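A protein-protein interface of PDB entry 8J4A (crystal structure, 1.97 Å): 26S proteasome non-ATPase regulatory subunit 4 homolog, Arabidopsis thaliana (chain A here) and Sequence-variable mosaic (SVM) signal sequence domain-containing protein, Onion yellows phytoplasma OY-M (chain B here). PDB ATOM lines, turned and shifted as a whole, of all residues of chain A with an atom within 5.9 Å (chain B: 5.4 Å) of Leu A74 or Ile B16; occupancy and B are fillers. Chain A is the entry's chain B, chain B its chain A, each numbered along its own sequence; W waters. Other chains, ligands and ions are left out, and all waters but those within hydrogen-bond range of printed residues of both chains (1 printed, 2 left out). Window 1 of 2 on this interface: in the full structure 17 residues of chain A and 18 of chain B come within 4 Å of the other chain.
Of the printed residues of chain B, Leu A74 touches Val B14, Ile B16, Phe B27, Phe B30 and Tyr B96.
Ile B16 touches just these residues of chain A: Asn A35 and Leu A74.
Of the printed residues of chain A, Val B14 touches Gly A71, Leu A74 and Ala A75.
Of the printed residues of chain B, Asn A35 touches Ile B16 and Phe B27.
Of the printed residues of chain A, Asn B15 touches His A78.
Phe B18 touches none of the printed residues of chain A.
Met A77 touches none of the printed residues of chain B.
The nearest printed residue of chain A that does not touch Val B14 is Lys A72 (5.6 Å).
Water W1 lies within hydrogen-bond range of OG1 of Thr B17 (2.5 Å), ND1 of His A78 (2.7 Å) and O of Asn B15 (3.5 Å).
Of the 11 printed residues of chain B, 6 touch a printed residue of chain A.
Hydrophobic or aromatic side chains of chain B within 4 Å of the printed part of chain A: Val B14, Ile B16, Phe B27, Phe B30 and Tyr B96.
Of the 15 printed residues of chain A, 6 touch a printed residue of chain B.
Hydrophobic or aromatic side chains of chain A within 4 Å of the printed part of chain B: Leu A74 and His A78.
Among the printed residues, 12 pairs touch across the chains.
Among the printed residues, no Asp or Glu carboxylate lies within 4 Å of a Lys or Arg side-chain nitrogen of the other chain.
N of Gly A71 sits close to OH of Tyr B96, at 3.3 Å.
O of Val B14 lies within hydrogen-bond range of N of Ile B97 (2.8 Å).
The side-chain amide oxygen of Asn B15 lies within hydrogen-bond range of the indole nitrogen of Trp B99 (2.9 Å).
The backbone NH (N) of Ile B16 is in hydrogen-bond range of the backbone carbonyl oxygen (O) of Ile B97 (2.9 Å).
O of Ile B16 sits at hydrogen-bond distance from N of Trp B99, 2.8 Å away.
OD1 of Asp A69 lies close to N of Gly A71.
Among the printed residues, merely in contact across the chains: Asn A35 with Ile B16 (3.7 Å), Asn A35 with Phe B27 (3.2 Å), Leu A70 with Tyr B96 (3.9 Å), Gly A71 with Val B14 (3.8 Å), Leu A74 with Val B14 (3.7 Å), Leu A74 with Ile B16 (3.7 Å), Leu A74 with Phe B27 (3.7 Å), Leu A74 with Phe B30 (3.8 Å), Leu A74 with Tyr B96 (3.9 Å), Ala A75 with Val B14 (3.8 Å) and His A78 with Asn B15 (3.6 Å).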
ATOM      1  N   VAL A  34     -15.189 -31.048  18.064  1.00  0.00           N
ATOM      2  CA  VAL A  34     -15.386 -30.791  19.486  1.00  0.00           C
ATOM      3  C   VAL A  34     -14.803 -29.432  19.856  1.00  0.00           C
ATOM      4  O   VAL A  34     -15.428 -28.641  20.566  1.00  0.00           O
ATOM      5  CB  VAL A  34     -14.769 -31.921  20.331  1.00  0.00           C
ATOM      6  CG1 VAL A  34     -14.763 -31.535  21.789  1.00  0.00           C
ATOM      7  CG2 VAL A  34     -15.528 -33.238  20.107  1.00  0.00           C
ATOM      8  N   ASN A  35     -13.595 -29.138  19.378  1.00  0.00           N
ATOM      9  CA  ASN A  35     -13.009 -27.838  19.680  1.00  0.00           C
ATOM     10  C   ASN A  35     -13.914 -26.706  19.201  1.00  0.00           C
ATOM     11  O   ASN A  35     -14.189 -25.766  19.951  1.00  0.00           O
ATOM     12  CB  ASN A  35     -11.615 -27.733  19.066  1.00  0.00           C
ATOM     13  CG  ASN A  35     -10.604 -28.581  19.806  1.00  0.00           C
ATOM     14  OD1 ASN A  35     -10.797 -28.911  20.973  1.00  0.00           O
ATOM     15  ND2 ASN A  35      -9.544 -28.971  19.122  1.00  0.00           N
ATOM     16  N   CYS A  38     -16.997 -26.433  21.496  1.00  0.00           N
ATOM     17  CA  CYS A  38     -16.673 -25.824  22.779  1.00  0.00           C
ATOM     18  C   CYS A  38     -16.544 -24.307  22.651  1.00  0.00           C
ATOM     19  O   CYS A  38     -17.039 -23.557  23.499  1.00  0.00           O
ATOM     20  CB  CYS A  38     -15.380 -26.428  23.318  1.00  0.00           C
ATOM     21  SG  CYS A  38     -15.589 -28.143  23.928  1.00  0.00           S
ATOM     22  N   GLY A  39     -15.882 -23.840  21.593  1.00  0.00           N
ATOM     23  CA  GLY A  39     -15.784 -22.410  21.367  1.00  0.00           C
ATOM     24  C   GLY A  39     -17.141 -21.776  21.133  1.00  0.00           C
ATOM     25  O   GLY A  39     -17.450 -20.727  21.694  1.00  0.00           O
ATOM     26  N   ILE A  52     -16.539 -32.546  29.229  1.00  0.00           N
ATOM     27  CA  ILE A  52     -16.045 -33.505  28.248  1.00  0.00           C
ATOM     28  C   ILE A  52     -15.710 -34.831  28.936  1.00  0.00           C
ATOM     29  O   ILE A  52     -15.132 -34.867  30.029  1.00  0.00           O
ATOM     30  CB  ILE A  52     -14.834 -32.947  27.478  1.00  0.00           C
ATOM     31  CG1 ILE A  52     -15.270 -31.785  26.569  1.00  0.00           C
ATOM     32  CG2 ILE A  52     -14.200 -34.025  26.626  1.00  0.00           C
ATOM     33  CD1 ILE A  52     -14.105 -31.138  25.874  1.00  0.00           C
ATOM     34  N   ASP A  69     -14.647 -22.323  31.616  1.00  0.00           N
ATOM     35  CA  ASP A  69     -13.221 -22.057  31.419  1.00  0.00           C
ATOM     36  C   ASP A  69     -12.806 -22.720  30.107  1.00  0.00           C
ATOM     37  O   ASP A  69     -12.463 -23.904  30.059  1.00  0.00           O
ATOM     38  CB  ASP A  69     -12.441 -22.589  32.621  1.00  0.00           C
ATOM     39  CG  ASP A  69     -10.966 -22.135  32.674  1.00  0.00           C
ATOM     40  OD1 ASP A  69     -10.352 -21.820  31.628  1.00  0.00           O
ATOM     41  OD2 ASP A  69     -10.397 -22.169  33.800  1.00  0.00           O
ATOM     42  N   LEU A  70     -12.857 -21.939  29.019  1.00  0.00           N
ATOM     43  CA  LEU A  70     -12.556 -22.469  27.689  1.00  0.00           C
ATOM     44  C   LEU A  70     -11.148 -23.053  27.628  1.00  0.00           C
ATOM     45  O   LEU A  70     -10.925 -24.089  26.992  1.00  0.00           O
ATOM     46  CB  LEU A  70     -12.735 -21.379  26.627  1.00  0.00           C
ATOM     47  CG  LEU A  70     -12.476 -21.804  25.173  1.00  0.00           C
ATOM     48  CD1 LEU A  70     -13.378 -22.975  24.770  1.00  0.00           C
ATOM     49  CD2 LEU A  70     -12.639 -20.638  24.200  1.00  0.00           C
ATOM     50  N   GLY A  71     -10.192 -22.420  28.304  1.00  0.00           N
ATOM     51  CA  GLY A  71      -8.835 -22.945  28.289  1.00  0.00           C
ATOM     52  C   GLY A  71      -8.721 -24.301  28.963  1.00  0.00           C
ATOM     53  O   GLY A  71      -8.024 -25.191  28.466  1.00  0.00           O
ATOM     54  N   LYS A  72      -9.373 -24.464  30.116  1.00  0.00           N
ATOM     55  CA  LYS A  72      -9.403 -25.761  30.793  1.00  0.00           C
ATOM     56  C   LYS A  72     -10.040 -26.825  29.908  1.00  0.00           C
ATOM     57  O   LYS A  72      -9.560 -27.965  29.839  1.00  0.00           O
ATOM     58  CB  LYS A  72     -10.163 -25.628  32.119  1.00  0.00           C
ATOM     59  CG  LYS A  72     -10.229 -26.880  32.962  1.00  0.00           C
ATOM     60  CD  LYS A  72     -10.566 -26.520  34.402  1.00  0.00           C
ATOM     61  CE  LYS A  72     -10.522 -27.734  35.328  1.00  0.00           C
ATOM     62  NZ  LYS A  72     -11.885 -28.059  35.867  1.00  0.00           N
ATOM     63  N   ILE A  73     -11.091 -26.445  29.186  1.00  0.00           N
ATOM     64  CA  ILE A  73     -11.816 -27.363  28.312  1.00  0.00           C
ATOM     65  C   ILE A  73     -10.931 -27.814  27.167  1.00  0.00           C
ATOM     66  O   ILE A  73     -10.751 -29.015  26.935  1.00  0.00           O
ATOM     67  CB  ILE A  73     -13.085 -26.695  27.756  1.00  0.00           C
ATOM     68  CG1 ILE A  73     -14.124 -26.494  28.853  1.00  0.00           C
ATOM     69  CG2 ILE A  73     -13.641 -27.541  26.597  1.00  0.00           C
ATOM     70  CD1 ILE A  73     -15.166 -25.421  28.520  1.00  0.00           C
ATOM     71  N   LEU A  74     -10.401 -26.844  26.406  1.00  0.00           N
ATOM     72  CA  LEU A  74      -9.607 -27.165  25.226  1.00  0.00           C
ATOM     73  C   LEU A  74      -8.343 -27.930  25.597  1.00  0.00           C
ATOM     74  O   LEU A  74      -7.835 -28.709  24.786  1.00  0.00           O
ATOM     75  CB  LEU A  74      -9.248 -25.878  24.473  1.00  0.00           C
ATOM     76  CG  LEU A  74     -10.417 -25.109  23.860  1.00  0.00           C
ATOM     77  CD1 LEU A  74      -9.889 -23.933  23.034  1.00  0.00           C
ATOM     78  CD2 LEU A  74     -11.245 -26.049  22.998  1.00  0.00           C
ATOM     79  N   ALA A  75      -7.826 -27.731  26.809  1.00  0.00           N
ATOM     80  CA  ALA A  75      -6.618 -28.446  27.227  1.00  0.00           C
ATOM     81  C   ALA A  75      -6.841 -29.948  27.361  1.00  0.00           C
ATOM     82  O   ALA A  75      -5.872 -30.720  27.243  1.00  0.00           O
ATOM     83  CB  ALA A  75      -6.089 -27.886  28.549  1.00  0.00           C
ATOM     84  N   CYS A  76      -8.091 -30.371  27.577  1.00  0.00           N
ATOM     85  CA  CYS A  76      -8.431 -31.784  27.675  1.00  0.00           C
ATOM     86  C   CYS A  76      -8.280 -32.512  26.349  1.00  0.00           C
ATOM     87  O   CYS A  76      -8.177 -33.742  26.342  1.00  0.00           O
ATOM     88  CB  CYS A  76      -9.877 -31.949  28.137  1.00  0.00           C
ATOM     89  SG  CYS A  76     -10.232 -31.248  29.730  1.00  0.00           S
ATOM     90  N   MET A  77      -8.295 -31.793  25.228  1.00  0.00           N
ATOM     91  CA  MET A  77      -8.375 -32.431  23.922  1.00  0.00           C
ATOM     92  C   MET A  77      -7.014 -32.669  23.281  1.00  0.00           C
ATOM     93  O   MET A  77      -6.957 -33.150  22.147  1.00  0.00           O
ATOM     94  CB  MET A  77      -9.274 -31.604  22.994  1.00  0.00           C
ATOM     95  CG  MET A  77     -10.734 -31.509  23.481  1.00  0.00           C
ATOM     96  SD  MET A  77     -11.534 -33.141  23.535  1.00  0.00           S
ATOM     97  CE  MET A  77     -11.295 -33.604  21.813  1.00  0.00           C
ATOM     98  N   HIS A  78      -5.921 -32.373  23.981  1.00  0.00           N
ATOM     99  CA  HIS A  78      -4.582 -32.666  23.489  1.00  0.00           C
ATOM    100  C   HIS A  78      -4.039 -33.899  24.202  1.00  0.00           C
ATOM    101  O   HIS A  78      -4.057 -33.967  25.436  1.00  0.00           O
ATOM    102  CB  HIS A  78      -3.642 -31.482  23.703  1.00  0.00           C
ATOM    103  CG  HIS A  78      -2.264 -31.712  23.168  1.00  0.00           C
ATOM    104  ND1 HIS A  78      -1.907 -31.394  21.878  1.00  0.00           N
ATOM    105  CD2 HIS A  78      -1.156 -32.233  23.747  1.00  0.00           C
ATOM    106  CE1 HIS A  78      -0.640 -31.713  21.680  1.00  0.00           C
ATOM    107  NE2 HIS A  78      -0.161 -32.226  22.798  1.00  0.00           N
ATOM    108  N   VAL B  14      -2.129 -24.333  25.913  1.00  0.00           N
ATOM    109  CA  VAL B  14      -3.177 -25.094  25.246  1.00  0.00           C
ATOM    110  C   VAL B  14      -2.776 -25.273  23.784  1.00  0.00           C
ATOM    111  O   VAL B  14      -2.768 -24.314  23.004  1.00  0.00           O
ATOM    112  CB  VAL B  14      -4.547 -24.404  25.356  1.00  0.00           C
ATOM    113  CG1 VAL B  14      -5.631 -25.322  24.830  1.00  0.00           C
ATOM    114  CG2 VAL B  14      -4.852 -24.000  26.812  1.00  0.00           C
ATOM    115  N   ASN B  15      -2.455 -26.505  23.408  1.00  0.00           N
ATOM    116  CA  ASN B  15      -2.046 -26.845  22.055  1.00  0.00           C
ATOM    117  C   ASN B  15      -3.285 -27.330  21.325  1.00  0.00           C
ATOM    118  O   ASN B  15      -3.978 -28.229  21.812  1.00  0.00           O
ATOM    119  CB  ASN B  15      -0.951 -27.920  22.058  1.00  0.00           C
ATOM    120  CG  ASN B  15       0.361 -27.421  22.655  1.00  0.00           C
ATOM    121  OD1 ASN B  15       1.129 -26.734  21.986  1.00  0.00           O
ATOM    122  ND2 ASN B  15       0.614 -27.753  23.927  1.00  0.00           N
ATOM    123  N   ILE B  16      -3.593 -26.698  20.193  1.00  0.00           N
ATOM    124  CA  ILE B  16      -4.768 -27.021  19.395  1.00  0.00           C
ATOM    125  C   ILE B  16      -4.277 -27.313  17.990  1.00  0.00           C
ATOM    126  O   ILE B  16      -3.430 -26.575  17.469  1.00  0.00           O
ATOM    127  CB  ILE B  16      -5.803 -25.869  19.389  1.00  0.00           C
ATOM    128  CG1 ILE B  16      -6.218 -25.504  20.817  1.00  0.00           C
ATOM    129  CG2 ILE B  16      -7.033 -26.261  18.579  1.00  0.00           C
ATOM    130  CD1 ILE B  16      -6.752 -24.090  20.991  1.00  0.00           C
ATOM    131  N   THR B  17      -4.795 -28.385  17.380  1.00  0.00           N
ATOM    132  CA  THR B  17      -4.333 -28.814  16.068  1.00  0.00           C
ATOM    133  C   THR B  17      -5.498 -28.931  15.096  1.00  0.00           C
ATOM    134  O   THR B  17      -6.534 -29.517  15.425  1.00  0.00           O
ATOM    135  CB  THR B  17      -3.583 -30.150  16.151  1.00  0.00           C
ATOM    136  OG1 THR B  17      -2.584 -30.068  17.176  1.00  0.00           O
ATOM    137  CG2 THR B  17      -2.905 -30.445  14.827  1.00  0.00           C
ATOM    138  N   PHE B  18      -5.306 -28.389  13.893  1.00  0.00           N
ATOM    139  CA  PHE B  18      -6.289 -28.422  12.820  1.00  0.00           C
ATOM    140  C   PHE B  18      -5.627 -28.871  11.524  1.00  0.00           C
ATOM    141  O   PHE B  18      -4.478 -28.520  11.249  1.00  0.00           O
ATOM    142  CB  PHE B  18      -6.911 -27.032  12.589  1.00  0.00           C
ATOM    143  CG  PHE B  18      -7.924 -26.623  13.631  1.00  0.00           C
ATOM    144  CD1 PHE B  18      -9.198 -27.161  13.624  1.00  0.00           C
ATOM    145  CD2 PHE B  18      -7.615 -25.662  14.573  1.00  0.00           C
ATOM    146  CE1 PHE B  18     -10.139 -26.772  14.551  1.00  0.00           C
ATOM    147  CE2 PHE B  18      -8.549 -25.263  15.502  1.00  0.00           C
ATOM    148  CZ  PHE B  18      -9.811 -25.827  15.499  1.00  0.00           C
ATOM    149  N   PHE B  27     -13.794 -20.766  14.429  1.00  0.00           N
ATOM    150  CA  PHE B  27     -13.446 -21.166  15.792  1.00  0.00           C
ATOM    151  C   PHE B  27     -13.565 -19.930  16.676  1.00  0.00           C
ATOM    152  O   PHE B  27     -12.662 -19.091  16.713  1.00  0.00           O
ATOM    153  CB  PHE B  27     -12.046 -21.767  15.810  1.00  0.00           C
ATOM    154  CG  PHE B  27     -11.664 -22.421  17.106  1.00  0.00           C
ATOM    155  CD1 PHE B  27     -12.608 -22.676  18.087  1.00  0.00           C
ATOM    156  CD2 PHE B  27     -10.340 -22.793  17.335  1.00  0.00           C
ATOM    157  CE1 PHE B  27     -12.238 -23.278  19.290  1.00  0.00           C
ATOM    158  CE2 PHE B  27      -9.961 -23.412  18.537  1.00  0.00           C
ATOM    159  CZ  PHE B  27     -10.912 -23.656  19.507  1.00  0.00           C
ATOM    160  N   PHE B  30     -11.414 -17.250  18.650  1.00  0.00           N
ATOM    161  CA  PHE B  30     -10.095 -17.093  18.055  1.00  0.00           C
ATOM    162  C   PHE B  30     -10.145 -16.562  16.637  1.00  0.00           C
ATOM    163  O   PHE B  30      -9.175 -15.947  16.183  1.00  0.00           O
ATOM    164  CB  PHE B  30      -9.386 -18.434  18.085  1.00  0.00           C
ATOM    165  CG  PHE B  30      -9.327 -19.018  19.457  1.00  0.00           C
ATOM    166  CD1 PHE B  30      -8.657 -18.353  20.464  1.00  0.00           C
ATOM    167  CD2 PHE B  30      -9.930 -20.213  19.740  1.00  0.00           C
ATOM    168  CE1 PHE B  30      -8.589 -18.886  21.734  1.00  0.00           C
ATOM    169  CE2 PHE B  30      -9.855 -20.744  21.012  1.00  0.00           C
ATOM    170  CZ  PHE B  30      -9.202 -20.070  21.997  1.00  0.00           C
ATOM    171  N   TYR B  96      -2.586 -19.995  23.867  1.00  0.00           N
ATOM    172  CA  TYR B  96      -3.099 -20.902  22.852  1.00  0.00           C
ATOM    173  C   TYR B  96      -2.084 -21.026  21.726  1.00  0.00           C
ATOM    174  O   TYR B  96      -1.664 -20.022  21.143  1.00  0.00           O
ATOM    175  CB  TYR B  96      -4.429 -20.389  22.317  1.00  0.00           C
ATOM    176  CG  TYR B  96      -5.513 -20.405  23.365  1.00  0.00           C
ATOM    177  CD1 TYR B  96      -6.262 -21.567  23.607  1.00  0.00           C
ATOM    178  CD2 TYR B  96      -5.768 -19.273  24.152  1.00  0.00           C
ATOM    179  CE1 TYR B  96      -7.247 -21.589  24.589  1.00  0.00           C
ATOM    180  CE2 TYR B  96      -6.749 -19.284  25.133  1.00  0.00           C
ATOM    181  CZ  TYR B  96      -7.499 -20.437  25.337  1.00  0.00           C
ATOM    182  OH  TYR B  96      -8.491 -20.447  26.311  1.00  0.00           O
ATOM    183  N   ILE B  97      -1.675 -22.247  21.432  1.00  0.00           N
ATOM    184  CA  ILE B  97      -0.737 -22.484  20.348  1.00  0.00           C
ATOM    185  C   ILE B  97      -1.477 -23.310  19.330  1.00  0.00           C
ATOM    186  O   ILE B  97      -2.003 -24.382  19.665  1.00  0.00           O
ATOM    187  CB  ILE B  97       0.546 -23.172  20.837  1.00  0.00           C
ATOM    188  CG1 ILE B  97       1.169 -22.307  21.928  1.00  0.00           C
ATOM    189  CG2 ILE B  97       1.545 -23.355  19.673  1.00  0.00           C
ATOM    190  CD1 ILE B  97       2.358 -22.995  22.664  1.00  0.00           C
ATOM    191  N   PHE B  98      -1.534 -22.808  18.102  1.00  0.00           N
ATOM    192  CA  PHE B  98      -2.307 -23.431  17.036  1.00  0.00           C
ATOM    193  C   PHE B  98      -1.355 -24.096  16.065  1.00  0.00           C
ATOM    194  O   PHE B  98      -0.418 -23.450  15.583  1.00  0.00           O
ATOM    195  CB  PHE B  98      -3.156 -22.408  16.288  1.00  0.00           C
ATOM    196  CG  PHE B  98      -4.190 -21.753  17.140  1.00  0.00           C
ATOM    197  CD1 PHE B  98      -3.872 -20.654  17.926  1.00  0.00           C
ATOM    198  CD2 PHE B  98      -5.483 -22.234  17.148  1.00  0.00           C
ATOM    199  CE1 PHE B  98      -4.844 -20.064  18.742  1.00  0.00           C
ATOM    200  CE2 PHE B  98      -6.451 -21.639  17.933  1.00  0.00           C
ATOM    201  CZ  PHE B  98      -6.128 -20.548  18.728  1.00  0.00           C
ATOM    202  N   TRP B  99      -1.633 -25.367  15.761  1.00  0.00           N
ATOM    203  CA  TRP B  99      -0.780 -26.227  14.955  1.00  0.00           C
ATOM    204  C   TRP B  99      -1.555 -26.774  13.768  1.00  0.00           C
ATOM    205  O   TRP B  99      -2.757 -27.002  13.852  1.00  0.00           O
ATOM    206  CB  TRP B  99      -0.264 -27.410  15.745  1.00  0.00           C
ATOM    207  CG  TRP B  99       0.545 -27.055  16.937  1.00  0.00           C
ATOM    208  CD1 TRP B  99       0.115 -26.968  18.223  1.00  0.00           C
ATOM    209  CD2 TRP B  99       1.935 -26.747  16.950  1.00  0.00           C
ATOM    210  NE1 TRP B  99       1.158 -26.621  19.050  1.00  0.00           N
ATOM    211  CE2 TRP B  99       2.289 -26.480  18.287  1.00  0.00           C
ATOM    212  CE3 TRP B  99       2.919 -26.670  15.954  1.00  0.00           C
ATOM    213  CZ2 TRP B  99       3.584 -26.156  18.660  1.00  0.00           C
ATOM    214  CZ3 TRP B  99       4.202 -26.339  16.321  1.00  0.00           C
ATOM    215  CH2 TRP B  99       4.531 -26.090  17.662  1.00  0.00           C
HETATM  216  O   HOH W   1      -3.196 -30.755  19.542  1.00  0.00           O
